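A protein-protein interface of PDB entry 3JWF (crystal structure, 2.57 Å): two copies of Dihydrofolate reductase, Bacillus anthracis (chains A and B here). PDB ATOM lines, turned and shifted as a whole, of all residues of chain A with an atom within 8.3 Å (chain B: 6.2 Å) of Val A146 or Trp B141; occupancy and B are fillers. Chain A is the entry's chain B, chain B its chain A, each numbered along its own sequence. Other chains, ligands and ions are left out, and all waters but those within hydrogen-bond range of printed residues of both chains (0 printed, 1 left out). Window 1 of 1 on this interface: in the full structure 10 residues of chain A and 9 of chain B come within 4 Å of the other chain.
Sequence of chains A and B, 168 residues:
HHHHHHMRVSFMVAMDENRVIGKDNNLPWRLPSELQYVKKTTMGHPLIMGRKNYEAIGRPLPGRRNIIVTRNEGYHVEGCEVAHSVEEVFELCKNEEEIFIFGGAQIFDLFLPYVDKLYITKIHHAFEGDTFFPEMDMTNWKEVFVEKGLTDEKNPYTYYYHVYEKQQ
Glu A143 touches Lys B142, but with the chains exchanged Lys A142 does not touch Glu B143 (12.8 Å).
Positions printed for both chains: 142, 143, 144 and 164.
The backbone carbonyl oxygen of Lys B142 is in hydrogen-bond range of the backbone NH of Glu B165 (3.0 Å).
O of Asn B140 sits at hydrogen-bond distance from N of Gln B167 (2.8 Å).
The backbone carbonyl oxygen (O) of Glu A147 lies within hydrogen-bond range of the backbone NH (N) of Tyr A161 (2.8 Å).
The backbone NH (N) of Val A144 is in hydrogen-bond range of the backbone carbonyl oxygen (O) of Val A163.
A ring nitrogen (ND1) of His A162 is in hydrogen-bond range of the side-chain carboxylate (OE1) of Glu A143 (2.6 Å).
The backbone carbonyl oxygen of Leu B118 is in hydrogen-bond range of the backbone NH of Tyr B164, 2.8 Å away.
NZ of Lys B142 lies within salt-bridge range of OE2 of Glu A143.
The backbone NH (N) of Asn B140 is in hydrogen-bond range of the backbone carbonyl oxygen (O) of Val A144 (2.6 Å).
The backbone NH (N) of Glu B143 is in hydrogen-bond range of the backbone carbonyl oxygen (O) of Val A146.
O of Val A144 is in hydrogen-bond range of N of Trp B141, 3.3 Å away.
The side-chain carboxylate (OE2) of Glu B143 sits at hydrogen-bond distance from the backbone NH (N) of Lys A148 (3.0 Å).
The side-chain amide oxygen (OD1) of Asn B140 is in hydrogen-bond range of the side-chain amino group (NZ) of Lys A142, at 3.1 Å.
The side-chain carboxylate (OE1) of Glu A147 is in hydrogen-bond range of the side-chain hydroxyl (OH) of Tyr B164 (2.7 Å).
Printed residues of chain A that touch a printed residue of chain B: Lys A142, Glu A143, Val A144, Phe A145, Val A146, Glu A147 and Lys A148.
Hydrophobic or aromatic side chains of chain A within 4 Å of the printed part of chain B: Val A144, Phe A145 and Val A146.
Among the printed residues, 14 pairs touch across the chains.
Among the printed residues, Asp or Glu carboxylates within 4 Å of a Lys or Arg side-chain nitrogen of the other chain: Glu A143 with Lys B142.
Of the printed residues of chain B, Val A146 touches Trp B141 (3.9 Å), Lys B142 (3.7 Å) and Glu B143 (3.0 Å).
Of the printed residues of chain A, Trp B141 touches Val A144, Phe A145 and Val A146.
Of the printed residues of chain B, Glu A143 touches Lys B142 (3.4 Å).
Of the printed residues of chain A, Asn B140 touches Lys A142 and Val A144.
Of the printed residues of chain B, Phe A145 touches Met B138 and Trp B141.
Of the printed residues of chain A, Met B138 touches Val A144 and Phe A145.
Val A163 touches none of the printed residues of chain B.
The nearest residue of chain A that does not touch Trp B141 is Glu A143 (6.3 Å).
Met B138 touches Val A144.
O of Val A144 touches C of Thr B139 (3.6 Å).
Met B138 touches Phe A145.
Trp B141 touches Phe A145 (O to CD1, 3.3 Å).
Val A146 touches Trp B141.
Lys B142 touches Val A146 (CG to CG1, 3.7 Å).
Glu A147 touches Glu B143.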
ATOM      1  N   ILE A 120      -1.624   6.333  -1.556  1.00  0.00           N
ATOM      2  CA  ILE A 120      -1.382   5.706  -0.270  1.00  0.00           C
ATOM      3  C   ILE A 120      -2.584   5.807   0.667  1.00  0.00           C
ATOM      4  O   ILE A 120      -3.063   6.906   0.975  1.00  0.00           O
ATOM      5  CB  ILE A 120      -0.071   6.243   0.389  1.00  0.00           C
ATOM      6  CG1 ILE A 120       0.206   5.538   1.713  1.00  0.00           C
ATOM      7  CG2 ILE A 120      -0.113   7.756   0.575  1.00  0.00           C
ATOM      8  CD1 ILE A 120       1.671   5.459   2.032  1.00  0.00           C
ATOM      9  N   LYS A 122      -3.832   5.412   4.366  1.00  0.00           N
ATOM     10  CA  LYS A 122      -3.331   5.411   5.731  1.00  0.00           C
ATOM     11  C   LYS A 122      -4.387   4.880   6.693  1.00  0.00           C
ATOM     12  O   LYS A 122      -5.496   5.399   6.749  1.00  0.00           O
ATOM     13  CB  LYS A 122      -2.856   6.815   6.127  1.00  0.00           C
ATOM     14  CG  LYS A 122      -1.622   7.256   5.357  1.00  0.00           C
ATOM     15  CD  LYS A 122      -1.208   8.672   5.696  1.00  0.00           C
ATOM     16  CE  LYS A 122      -0.017   9.103   4.856  1.00  0.00           C
ATOM     17  NZ  LYS A 122       0.425  10.479   5.227  1.00  0.00           N
ATOM     18  N   LYS A 142       3.657  16.929  -3.485  1.00  0.00           N
ATOM     19  CA  LYS A 142       2.456  17.696  -3.206  1.00  0.00           C
ATOM     20  C   LYS A 142       1.264  16.750  -3.031  1.00  0.00           C
ATOM     21  O   LYS A 142       1.066  15.853  -3.855  1.00  0.00           O
ATOM     22  CB  LYS A 142       2.215  18.688  -4.348  1.00  0.00           C
ATOM     23  CG  LYS A 142       0.979  19.563  -4.226  1.00  0.00           C
ATOM     24  CD  LYS A 142       1.226  20.916  -4.887  1.00  0.00           C
ATOM     25  CE  LYS A 142      -0.066  21.560  -5.369  1.00  0.00           C
ATOM     26  NZ  LYS A 142      -0.445  21.039  -6.713  1.00  0.00           N
ATOM     27  N   GLU A 143       0.491  16.933  -1.956  1.00  0.00           N
ATOM     28  CA  GLU A 143      -0.760  16.193  -1.788  1.00  0.00           C
ATOM     29  C   GLU A 143      -1.829  16.781  -2.712  1.00  0.00           C
ATOM     30  O   GLU A 143      -2.230  17.938  -2.562  1.00  0.00           O
ATOM     31  CB  GLU A 143      -1.237  16.215  -0.332  1.00  0.00           C
ATOM     32  CG  GLU A 143      -2.366  15.221  -0.038  1.00  0.00           C
ATOM     33  CD  GLU A 143      -2.889  15.318   1.383  1.00  0.00           C
ATOM     34  OE1 GLU A 143      -2.822  14.305   2.109  1.00  0.00           O
ATOM     35  OE2 GLU A 143      -3.365  16.401   1.785  1.00  0.00           O
ATOM     36  N   VAL A 144      -2.283  15.978  -3.668  1.00  0.00           N
ATOM     37  CA  VAL A 144      -3.247  16.434  -4.663  1.00  0.00           C
ATOM     38  C   VAL A 144      -4.661  15.889  -4.407  1.00  0.00           C
ATOM     39  O   VAL A 144      -5.607  16.259  -5.101  1.00  0.00           O
ATOM     40  CB  VAL A 144      -2.780  16.087  -6.096  1.00  0.00           C
ATOM     41  CG1 VAL A 144      -1.546  16.909  -6.482  1.00  0.00           C
ATOM     42  CG2 VAL A 144      -2.514  14.589  -6.239  1.00  0.00           C
ATOM     43  N   PHE A 145      -4.790  15.016  -3.408  1.00  0.00           N
ATOM     44  CA  PHE A 145      -6.080  14.447  -3.030  1.00  0.00           C
ATOM     45  C   PHE A 145      -6.057  13.839  -1.629  1.00  0.00           C
ATOM     46  O   PHE A 145      -5.077  13.207  -1.230  1.00  0.00           O
ATOM     47  CB  PHE A 145      -6.545  13.397  -4.053  1.00  0.00           C
ATOM     48  CG  PHE A 145      -7.943  12.894  -3.813  1.00  0.00           C
ATOM     49  CD1 PHE A 145      -9.045  13.701  -4.079  1.00  0.00           C
ATOM     50  CD2 PHE A 145      -8.156  11.616  -3.312  1.00  0.00           C
ATOM     51  CE1 PHE A 145     -10.340  13.244  -3.855  1.00  0.00           C
ATOM     52  CE2 PHE A 145      -9.447  11.148  -3.083  1.00  0.00           C
ATOM     53  CZ  PHE A 145     -10.543  11.966  -3.360  1.00  0.00           C
ATOM     54  N   VAL A 146      -7.149  14.046  -0.895  1.00  0.00           N
ATOM     55  CA  VAL A 146      -7.380  13.404   0.401  1.00  0.00           C
ATOM     56  C   VAL A 146      -8.885  13.247   0.668  1.00  0.00           C
ATOM     57  O   VAL A 146      -9.667  14.166   0.412  1.00  0.00           O
ATOM     58  CB  VAL A 146      -6.665  14.158   1.569  1.00  0.00           C
ATOM     59  CG1 VAL A 146      -7.180  15.588   1.716  1.00  0.00           C
ATOM     60  CG2 VAL A 146      -6.797  13.385   2.884  1.00  0.00           C
ATOM     61  N   GLU A 147      -9.287  12.072   1.146  1.00  0.00           N
ATOM     62  CA  GLU A 147     -10.669  11.845   1.595  1.00  0.00           C
ATOM     63  C   GLU A 147     -10.770  10.705   2.614  1.00  0.00           C
ATOM     64  O   GLU A 147      -9.986   9.744   2.583  1.00  0.00           O
ATOM     65  CB  GLU A 147     -11.644  11.626   0.418  1.00  0.00           C
ATOM     66  CG  GLU A 147     -11.755  10.179  -0.073  1.00  0.00           C
ATOM     67  CD  GLU A 147     -12.842   9.960  -1.117  1.00  0.00           C
ATOM     68  OE1 GLU A 147     -13.472  10.945  -1.551  1.00  0.00           O
ATOM     69  OE2 GLU A 147     -13.061   8.789  -1.510  1.00  0.00           O
ATOM     70  N   LYS A 148     -11.740  10.829   3.515  1.00  0.00           N
ATOM     71  CA  LYS A 148     -11.997   9.810   4.516  1.00  0.00           C
ATOM     72  C   LYS A 148     -12.574   8.565   3.856  1.00  0.00           C
ATOM     73  O   LYS A 148     -13.472   8.654   3.026  1.00  0.00           O
ATOM     74  CB  LYS A 148     -12.948  10.343   5.588  1.00  0.00           C
ATOM     75  CG  LYS A 148     -12.863   9.609   6.909  1.00  0.00           C
ATOM     76  CD  LYS A 148     -14.041   9.930   7.812  1.00  0.00           C
ATOM     77  CE  LYS A 148     -13.841   9.361   9.212  1.00  0.00           C
ATOM     78  NZ  LYS A 148     -13.904   7.875   9.255  1.00  0.00           N
ATOM     79  N   GLY A 149     -12.034   7.409   4.217  1.00  0.00           N
ATOM     80  CA  GLY A 149     -12.580   6.133   3.766  1.00  0.00           C
ATOM     81  C   GLY A 149     -13.828   5.755   4.549  1.00  0.00           C
ATOM     82  O   GLY A 149     -14.128   6.351   5.595  1.00  0.00           O
ATOM     83  N   TYR A 159      -9.632   5.170   8.240  1.00  0.00           N
ATOM     84  CA  TYR A 159      -8.596   5.279   7.209  1.00  0.00           C
ATOM     85  C   TYR A 159      -8.886   6.390   6.202  1.00  0.00           C
ATOM     86  O   TYR A 159     -10.044   6.768   5.979  1.00  0.00           O
ATOM     87  CB  TYR A 159      -8.383   3.936   6.482  1.00  0.00           C
ATOM     88  CG  TYR A 159      -9.586   3.401   5.728  1.00  0.00           C
ATOM     89  CD1 TYR A 159      -9.586   3.328   4.337  1.00  0.00           C
ATOM     90  CD2 TYR A 159     -10.719   2.945   6.412  1.00  0.00           C
ATOM     91  CE1 TYR A 159     -10.686   2.825   3.640  1.00  0.00           C
ATOM     92  CE2 TYR A 159     -11.821   2.449   5.732  1.00  0.00           C
ATOM     93  CZ  TYR A 159     -11.802   2.390   4.346  1.00  0.00           C
ATOM     94  OH  TYR A 159     -12.899   1.897   3.678  1.00  0.00           O
ATOM     95  N   TYR A 160      -7.821   6.908   5.598  1.00  0.00           N
ATOM     96  CA  TYR A 160      -7.923   7.995   4.633  1.00  0.00           C
ATOM     97  C   TYR A 160      -7.171   7.641   3.360  1.00  0.00           C
ATOM     98  O   TYR A 160      -6.139   6.967   3.406  1.00  0.00           O
ATOM     99  CB  TYR A 160      -7.354   9.289   5.231  1.00  0.00           C
ATOM    100  CG  TYR A 160      -8.210   9.901   6.315  1.00  0.00           C
ATOM    101  CD1 TYR A 160      -8.199   9.390   7.614  1.00  0.00           C
ATOM    102  CD2 TYR A 160      -9.021  11.001   6.045  1.00  0.00           C
ATOM    103  CE1 TYR A 160      -8.981   9.948   8.612  1.00  0.00           C
ATOM    104  CE2 TYR A 160      -9.812  11.570   7.036  1.00  0.00           C
ATOM    105  CZ  TYR A 160      -9.787  11.035   8.317  1.00  0.00           C
ATOM    106  OH  TYR A 160     -10.564  11.593   9.303  1.00  0.00           O
ATOM    107  N   TYR A 161      -7.699   8.091   2.226  1.00  0.00           N
ATOM    108  CA  TYR A 161      -6.996   7.972   0.955  1.00  0.00           C
ATOM    109  C   TYR A 161      -6.180   9.238   0.744  1.00  0.00           C
ATOM    110  O   TYR A 161      -6.689  10.341   0.936  1.00  0.00           O
ATOM    111  CB  TYR A 161      -7.963   7.813  -0.217  1.00  0.00           C
ATOM    112  CG  TYR A 161      -8.962   6.686  -0.089  1.00  0.00           C
ATOM    113  CD1 TYR A 161     -10.317   6.954   0.161  1.00  0.00           C
ATOM    114  CD2 TYR A 161      -8.566   5.357  -0.229  1.00  0.00           C
ATOM    115  CE1 TYR A 161     -11.247   5.928   0.271  1.00  0.00           C
ATOM    116  CE2 TYR A 161      -9.492   4.319  -0.117  1.00  0.00           C
ATOM    117  CZ  TYR A 161     -10.829   4.613   0.130  1.00  0.00           C
ATOM    118  OH  TYR A 161     -11.739   3.586   0.237  1.00  0.00           O
ATOM    119  N   HIS A 162      -4.913   9.069   0.366  1.00  0.00           N
ATOM    120  CA  HIS A 162      -4.049  10.189   0.011  1.00  0.00           C
ATOM    121  C   HIS A 162      -3.438   9.943  -1.361  1.00  0.00           C
ATOM    122  O   HIS A 162      -3.141   8.804  -1.728  1.00  0.00           O
ATOM    123  CB  HIS A 162      -2.924  10.377   1.028  1.00  0.00           C
ATOM    124  CG  HIS A 162      -3.384  10.661   2.427  1.00  0.00           C
ATOM    125  ND1 HIS A 162      -3.434  11.935   2.953  1.00  0.00           N
ATOM    126  CD2 HIS A 162      -3.769   9.830   3.425  1.00  0.00           C
ATOM    127  CE1 HIS A 162      -3.844  11.878   4.208  1.00  0.00           C
ATOM    128  NE2 HIS A 162      -4.054  10.612   4.518  1.00  0.00           N
ATOM    129  N   VAL A 163      -3.278  11.018  -2.123  1.00  0.00           N
ATOM    130  CA  VAL A 163      -2.534  10.971  -3.374  1.00  0.00           C
ATOM    131  C   VAL A 163      -1.498  12.097  -3.379  1.00  0.00           C
ATOM    132  O   VAL A 163      -1.813  13.260  -3.112  1.00  0.00           O
ATOM    133  CB  VAL A 163      -3.449  11.054  -4.630  1.00  0.00           C
ATOM    134  CG1 VAL A 163      -2.643  10.818  -5.891  1.00  0.00           C
ATOM    135  CG2 VAL A 163      -4.590  10.040  -4.553  1.00  0.00           C
ATOM    136  N   TYR A 164      -0.254  11.737  -3.666  1.00  0.00           N
ATOM    137  CA  TYR A 164       0.818  12.712  -3.749  1.00  0.00           C
ATOM    138  C   TYR A 164       1.451  12.665  -5.130  1.00  0.00           C
ATOM    139  O   TYR A 164       1.574  11.594  -5.731  1.00  0.00           O
ATOM    140  CB  TYR A 164       1.881  12.430  -2.694  1.00  0.00           C
ATOM    141  CG  TYR A 164       1.388  12.412  -1.267  1.00  0.00           C
ATOM    142  CD1 TYR A 164       1.464  13.554  -0.467  1.00  0.00           C
ATOM    143  CD2 TYR A 164       0.878  11.240  -0.705  1.00  0.00           C
ATOM    144  CE1 TYR A 164       1.026  13.534   0.857  1.00  0.00           C
ATOM    145  CE2 TYR A 164       0.441  11.205   0.611  1.00  0.00           C
ATOM    146  CZ  TYR A 164       0.513  12.350   1.388  1.00  0.00           C
ATOM    147  OH  TYR A 164       0.070  12.300   2.692  1.00  0.00           O
ATOM    148  N   VAL B 115     -16.306  24.799 -11.475  1.00  0.00           N
ATOM    149  CA  VAL B 115     -16.599  24.464 -10.076  1.00  0.00           C
ATOM    150  C   VAL B 115     -15.380  24.646  -9.151  1.00  0.00           C
ATOM    151  O   VAL B 115     -14.271  24.226  -9.488  1.00  0.00           O
ATOM    152  CB  VAL B 115     -17.242  23.045  -9.949  1.00  0.00           C
ATOM    153  CG1 VAL B 115     -16.271  21.947 -10.406  1.00  0.00           C
ATOM    154  CG2 VAL B 115     -17.758  22.789  -8.530  1.00  0.00           C
ATOM    155  N   ASP B 116     -15.610  25.299  -8.007  1.00  0.00           N
ATOM    156  CA  ASP B 116     -14.585  25.547  -6.978  1.00  0.00           C
ATOM    157  C   ASP B 116     -14.819  24.660  -5.764  1.00  0.00           C
ATOM    158  O   ASP B 116     -13.868  24.218  -5.110  1.00  0.00           O
ATOM    159  CB  ASP B 116     -14.612  27.007  -6.503  1.00  0.00           C
ATOM    160  CG  ASP B 116     -14.489  27.997  -7.638  1.00  0.00           C
ATOM    161  OD1 ASP B 116     -15.414  28.831  -7.791  1.00  0.00           O
ATOM    162  OD2 ASP B 116     -13.480  27.936  -8.382  1.00  0.00           O
ATOM    163  N   LYS B 117     -16.093  24.418  -5.460  1.00  0.00           N
ATOM    164  CA  LYS B 117     -16.485  23.703  -4.257  1.00  0.00           C
ATOM    165  C   LYS B 117     -17.602  22.705  -4.568  1.00  0.00           C
ATOM    166  O   LYS B 117     -18.528  23.003  -5.324  1.00  0.00           O
ATOM    167  CB  LYS B 117     -16.940  24.708  -3.200  1.00  0.00           C
ATOM    168  CG  LYS B 117     -16.875  24.208  -1.776  1.00  0.00           C
ATOM    169  CD  LYS B 117     -17.080  25.348  -0.783  1.00  0.00           C
ATOM    170  CE  LYS B 117     -16.670  24.920   0.615  1.00  0.00           C
ATOM    171  NZ  LYS B 117     -17.551  25.495   1.654  1.00  0.00           N
ATOM    172  N   LEU B 118     -17.517  21.521  -3.981  1.00  0.00           N
ATOM    173  CA  LEU B 118     -18.514  20.494  -4.217  1.00  0.00           C
ATOM    174  C   LEU B 118     -19.153  20.034  -2.906  1.00  0.00           C
ATOM    175  O   LEU B 118     -18.466  19.510  -2.025  1.00  0.00           O
ATOM    176  CB  LEU B 118     -17.877  19.311  -4.960  1.00  0.00           C
ATOM    177  CG  LEU B 118     -18.678  18.014  -5.118  1.00  0.00           C
ATOM    178  CD1 LEU B 118     -19.863  18.196  -6.059  1.00  0.00           C
ATOM    179  CD2 LEU B 118     -17.781  16.910  -5.622  1.00  0.00           C
ATOM    180  N   MET B 136     -15.932  13.176 -12.404  1.00  0.00           N
ATOM    181  CA  MET B 136     -15.058  14.265 -11.998  1.00  0.00           C
ATOM    182  C   MET B 136     -13.668  13.770 -11.623  1.00  0.00           C
ATOM    183  O   MET B 136     -13.515  12.902 -10.760  1.00  0.00           O
ATOM    184  CB  MET B 136     -15.651  15.002 -10.801  1.00  0.00           C
ATOM    185  CG  MET B 136     -16.770  15.971 -11.117  1.00  0.00           C
ATOM    186  SD  MET B 136     -17.168  16.976  -9.670  1.00  0.00           S
ATOM    187  CE  MET B 136     -15.623  17.842  -9.397  1.00  0.00           C
ATOM    188  N   ASP B 137     -12.664  14.340 -12.286  1.00  0.00           N
ATOM    189  CA  ASP B 137     -11.274  14.222 -11.877  1.00  0.00           C
ATOM    190  C   ASP B 137     -11.115  15.074 -10.624  1.00  0.00           C
ATOM    191  O   ASP B 137     -11.340  16.288 -10.657  1.00  0.00           O
ATOM    192  CB  ASP B 137     -10.362  14.738 -12.996  1.00  0.00           C
ATOM    193  CG  ASP B 137      -8.879  14.462 -12.743  1.00  0.00           C
ATOM    194  OD1 ASP B 137      -8.506  13.991 -11.643  1.00  0.00           O
ATOM    195  OD2 ASP B 137      -8.080  14.726 -13.670  1.00  0.00           O
ATOM    196  N   MET B 138     -10.742  14.428  -9.521  1.00  0.00           N
ATOM    197  CA  MET B 138     -10.603  15.107  -8.232  1.00  0.00           C
ATOM    198  C   MET B 138      -9.162  15.493  -7.912  1.00  0.00           C
ATOM    199  O   MET B 138      -8.878  15.981  -6.812  1.00  0.00           O
ATOM    200  CB  MET B 138     -11.185  14.262  -7.098  1.00  0.00           C
ATOM    201  CG  MET B 138     -12.681  13.985  -7.212  1.00  0.00           C
ATOM    202  SD  MET B 138     -13.718  15.462  -7.302  1.00  0.00           S
ATOM    203  CE  MET B 138     -13.735  15.996  -5.605  1.00  0.00           C
ATOM    204  N   THR B 139      -8.257  15.284  -8.868  1.00  0.00           N
ATOM    205  CA  THR B 139      -6.874  15.718  -8.713  1.00  0.00           C
ATOM    206  C   THR B 139      -6.880  17.200  -8.357  1.00  0.00           C
ATOM    207  O   THR B 139      -7.543  18.003  -9.014  1.00  0.00           O
ATOM    208  CB  THR B 139      -6.042  15.483  -9.994  1.00  0.00           C
ATOM    209  OG1 THR B 139      -6.340  14.190 -10.535  1.00  0.00           O
ATOM    210  CG2 THR B 139      -4.547  15.569  -9.697  1.00  0.00           C
ATOM    211  N   ASN B 140      -6.152  17.545  -7.301  1.00  0.00           N
ATOM    212  CA  ASN B 140      -6.118  18.909  -6.761  1.00  0.00           C
ATOM    213  C   ASN B 140      -7.411  19.344  -6.064  1.00  0.00           C
ATOM    214  O   ASN B 140      -7.711  20.540  -5.978  1.00  0.00           O
ATOM    215  CB  ASN B 140      -5.648  19.926  -7.816  1.00  0.00           C
ATOM    216  CG  ASN B 140      -4.177  19.759  -8.158  1.00  0.00           C
ATOM    217  OD1 ASN B 140      -3.299  20.090  -7.361  1.00  0.00           O
ATOM    218  ND2 ASN B 140      -3.902  19.221  -9.337  1.00  0.00           N
ATOM    219  N   TRP B 141      -8.161  18.359  -5.565  1.00  0.00           N
ATOM    220  CA  TRP B 141      -9.273  18.603  -4.645  1.00  0.00           C
ATOM    221  C   TRP B 141      -9.010  17.912  -3.317  1.00  0.00           C
ATOM    222  O   TRP B 141      -8.385  16.858  -3.274  1.00  0.00           O
ATOM    223  CB  TRP B 141     -10.585  18.079  -5.213  1.00  0.00           C
ATOM    224  CG  TRP B 141     -11.075  18.789  -6.429  1.00  0.00           C
ATOM    225  CD1 TRP B 141     -10.517  18.766  -7.676  1.00  0.00           C
ATOM    226  CD2 TRP B 141     -12.249  19.597  -6.530  1.00  0.00           C
ATOM    227  NE1 TRP B 141     -11.263  19.521  -8.543  1.00  0.00           N
ATOM    228  CE2 TRP B 141     -12.332  20.046  -7.868  1.00  0.00           C
ATOM    229  CE3 TRP B 141     -13.238  19.990  -5.621  1.00  0.00           C
ATOM    230  CZ2 TRP B 141     -13.365  20.871  -8.319  1.00  0.00           C
ATOM    231  CZ3 TRP B 141     -14.264  20.811  -6.070  1.00  0.00           C
ATOM    232  CH2 TRP B 141     -14.319  21.242  -7.409  1.00  0.00           C
ATOM    233  N   LYS B 142      -9.496  18.516  -2.237  1.00  0.00           N
ATOM    234  CA  LYS B 142      -9.394  17.940  -0.900  1.00  0.00           C
ATOM    235  C   LYS B 142     -10.749  17.965  -0.202  1.00  0.00           C
ATOM    236  O   LYS B 142     -11.463  18.971  -0.234  1.00  0.00           O
ATOM    237  CB  LYS B 142      -8.369  18.701  -0.058  1.00  0.00           C
ATOM    238  CG  LYS B 142      -6.942  18.550  -0.539  1.00  0.00           C
ATOM    239  CD  LYS B 142      -5.967  19.151   0.444  1.00  0.00           C
ATOM    240  CE  LYS B 142      -4.547  18.984  -0.047  1.00  0.00           C
ATOM    241  NZ  LYS B 142      -3.619  19.744   0.820  1.00  0.00           N
ATOM    242  N   GLU B 143     -11.097  16.850   0.426  1.00  0.00           N
ATOM    243  CA  GLU B 143     -12.298  16.766   1.244  1.00  0.00           C
ATOM    244  C   GLU B 143     -12.085  17.577   2.508  1.00  0.00           C
ATOM    245  O   GLU B 143     -11.144  17.328   3.259  1.00  0.00           O
ATOM    246  CB  GLU B 143     -12.587  15.312   1.602  1.00  0.00           C
ATOM    247  CG  GLU B 143     -13.891  15.073   2.347  1.00  0.00           C
ATOM    248  CD  GLU B 143     -13.943  13.691   2.977  1.00  0.00           C
ATOM    249  OE1 GLU B 143     -14.715  12.840   2.496  1.00  0.00           O
ATOM    250  OE2 GLU B 143     -13.197  13.450   3.953  1.00  0.00           O
ATOM    251  N   VAL B 144     -12.954  18.554   2.737  1.00  0.00           N
ATOM    252  CA  VAL B 144     -12.823  19.435   3.903  1.00  0.00           C
ATOM    253  C   VAL B 144     -13.924  19.193   4.934  1.00  0.00           C
ATOM    254  O   VAL B 144     -13.942  19.823   5.990  1.00  0.00           O
ATOM    255  CB  VAL B 144     -12.772  20.931   3.507  1.00  0.00           C
ATOM    256  CG1 VAL B 144     -11.639  21.180   2.516  1.00  0.00           C
ATOM    257  CG2 VAL B 144     -14.105  21.393   2.933  1.00  0.00           C
ATOM    258  N   TYR B 164     -15.990  19.054  -0.833  1.00  0.00           N
ATOM    259  CA  TYR B 164     -14.662  19.117  -1.432  1.00  0.00           C
ATOM    260  C   TYR B 164     -14.359  20.534  -1.890  1.00  0.00           C
ATOM    261  O   TYR B 164     -15.241  21.227  -2.396  1.00  0.00           O
ATOM    262  CB  TYR B 164     -14.566  18.184  -2.643  1.00  0.00           C
ATOM    263  CG  TYR B 164     -14.818  16.716  -2.365  1.00  0.00           C
ATOM    264  CD1 TYR B 164     -13.773  15.863  -1.996  1.00  0.00           C
ATOM    265  CD2 TYR B 164     -16.092  16.174  -2.506  1.00  0.00           C
ATOM    266  CE1 TYR B 164     -14.003  14.511  -1.756  1.00  0.00           C
ATOM    267  CE2 TYR B 164     -16.331  14.831  -2.276  1.00  0.00           C
ATOM    268  CZ  TYR B 164     -15.289  14.005  -1.898  1.00  0.00           C
ATOM    269  OH  TYR B 164     -15.543  12.673  -1.665  1.00  0.00           O
ATOM    270  N   GLU B 165     -13.105  20.946  -1.725  1.00  0.00           N
ATOM    271  CA  GLU B 165     -12.632  22.236  -2.214  1.00  0.00           C
ATOM    272  C   GLU B 165     -11.513  22.066  -3.226  1.00  0.00           C
ATOM    273  O   GLU B 165     -10.633  21.224  -3.054  1.00  0.00           O
ATOM    274  CB  GLU B 165     -12.128  23.102  -1.063  1.00  0.00           C
ATOM    275  CG  GLU B 165     -13.214  23.812  -0.281  1.00  0.00           C
ATOM    276  CD  GLU B 165     -12.659  24.694   0.830  1.00  0.00           C
ATOM    277  OE1 GLU B 165     -11.447  25.001   0.808  1.00  0.00           O
ATOM    278  OE2 GLU B 165     -13.441  25.080   1.727  1.00  0.00           O
ATOM    279  N   LYS B 166     -11.550  22.880  -4.276  1.00  0.00           N
ATOM    280  CA  LYS B 166     -10.485  22.920  -5.269  1.00  0.00           C
ATOM    281  C   LYS B 166      -9.275  23.626  -4.678  1.00  0.00           C
ATOM    282  O   LYS B 166      -9.427  24.565  -3.890  1.00  0.00           O
ATOM    283  CB  LYS B 166     -10.949  23.687  -6.501  1.00  0.00           C
ATOM    284  CG  LYS B 166     -10.268  23.273  -7.786  1.00  0.00           C
ATOM    285  CD  LYS B 166     -10.409  24.358  -8.839  1.00  0.00           C
ATOM    286  CE  LYS B 166     -10.616  23.766 -10.227  1.00  0.00           C
ATOM    287  NZ  LYS B 166      -9.635  22.691 -10.585  1.00  0.00           N
ATOM    288  N   GLN B 167      -8.083  23.167  -5.054  1.00  0.00           N
ATOM    289  CA  GLN B 167      -6.837  23.839  -4.675  1.00  0.00           C
ATOM    290  C   GLN B 167      -6.272  24.627  -5.868  1.00  0.00           C
ATOM    291  O   GLN B 167      -6.446  24.224  -7.025  1.00  0.00           O
ATOM    292  CB  GLN B 167      -5.804  22.831  -4.142  1.00  0.00           C
ATOM    293  CG  GLN B 167      -6.353  21.768  -3.166  1.00  0.00           C
ATOM    294  CD  GLN B 167      -6.844  22.338  -1.834  1.00  0.00           C
ATOM    295  OE1 GLN B 167      -6.106  23.016  -1.121  1.00  0.00           O
ATOM    296  NE2 GLN B 167      -8.094  22.043  -1.491  1.00  0.00           N
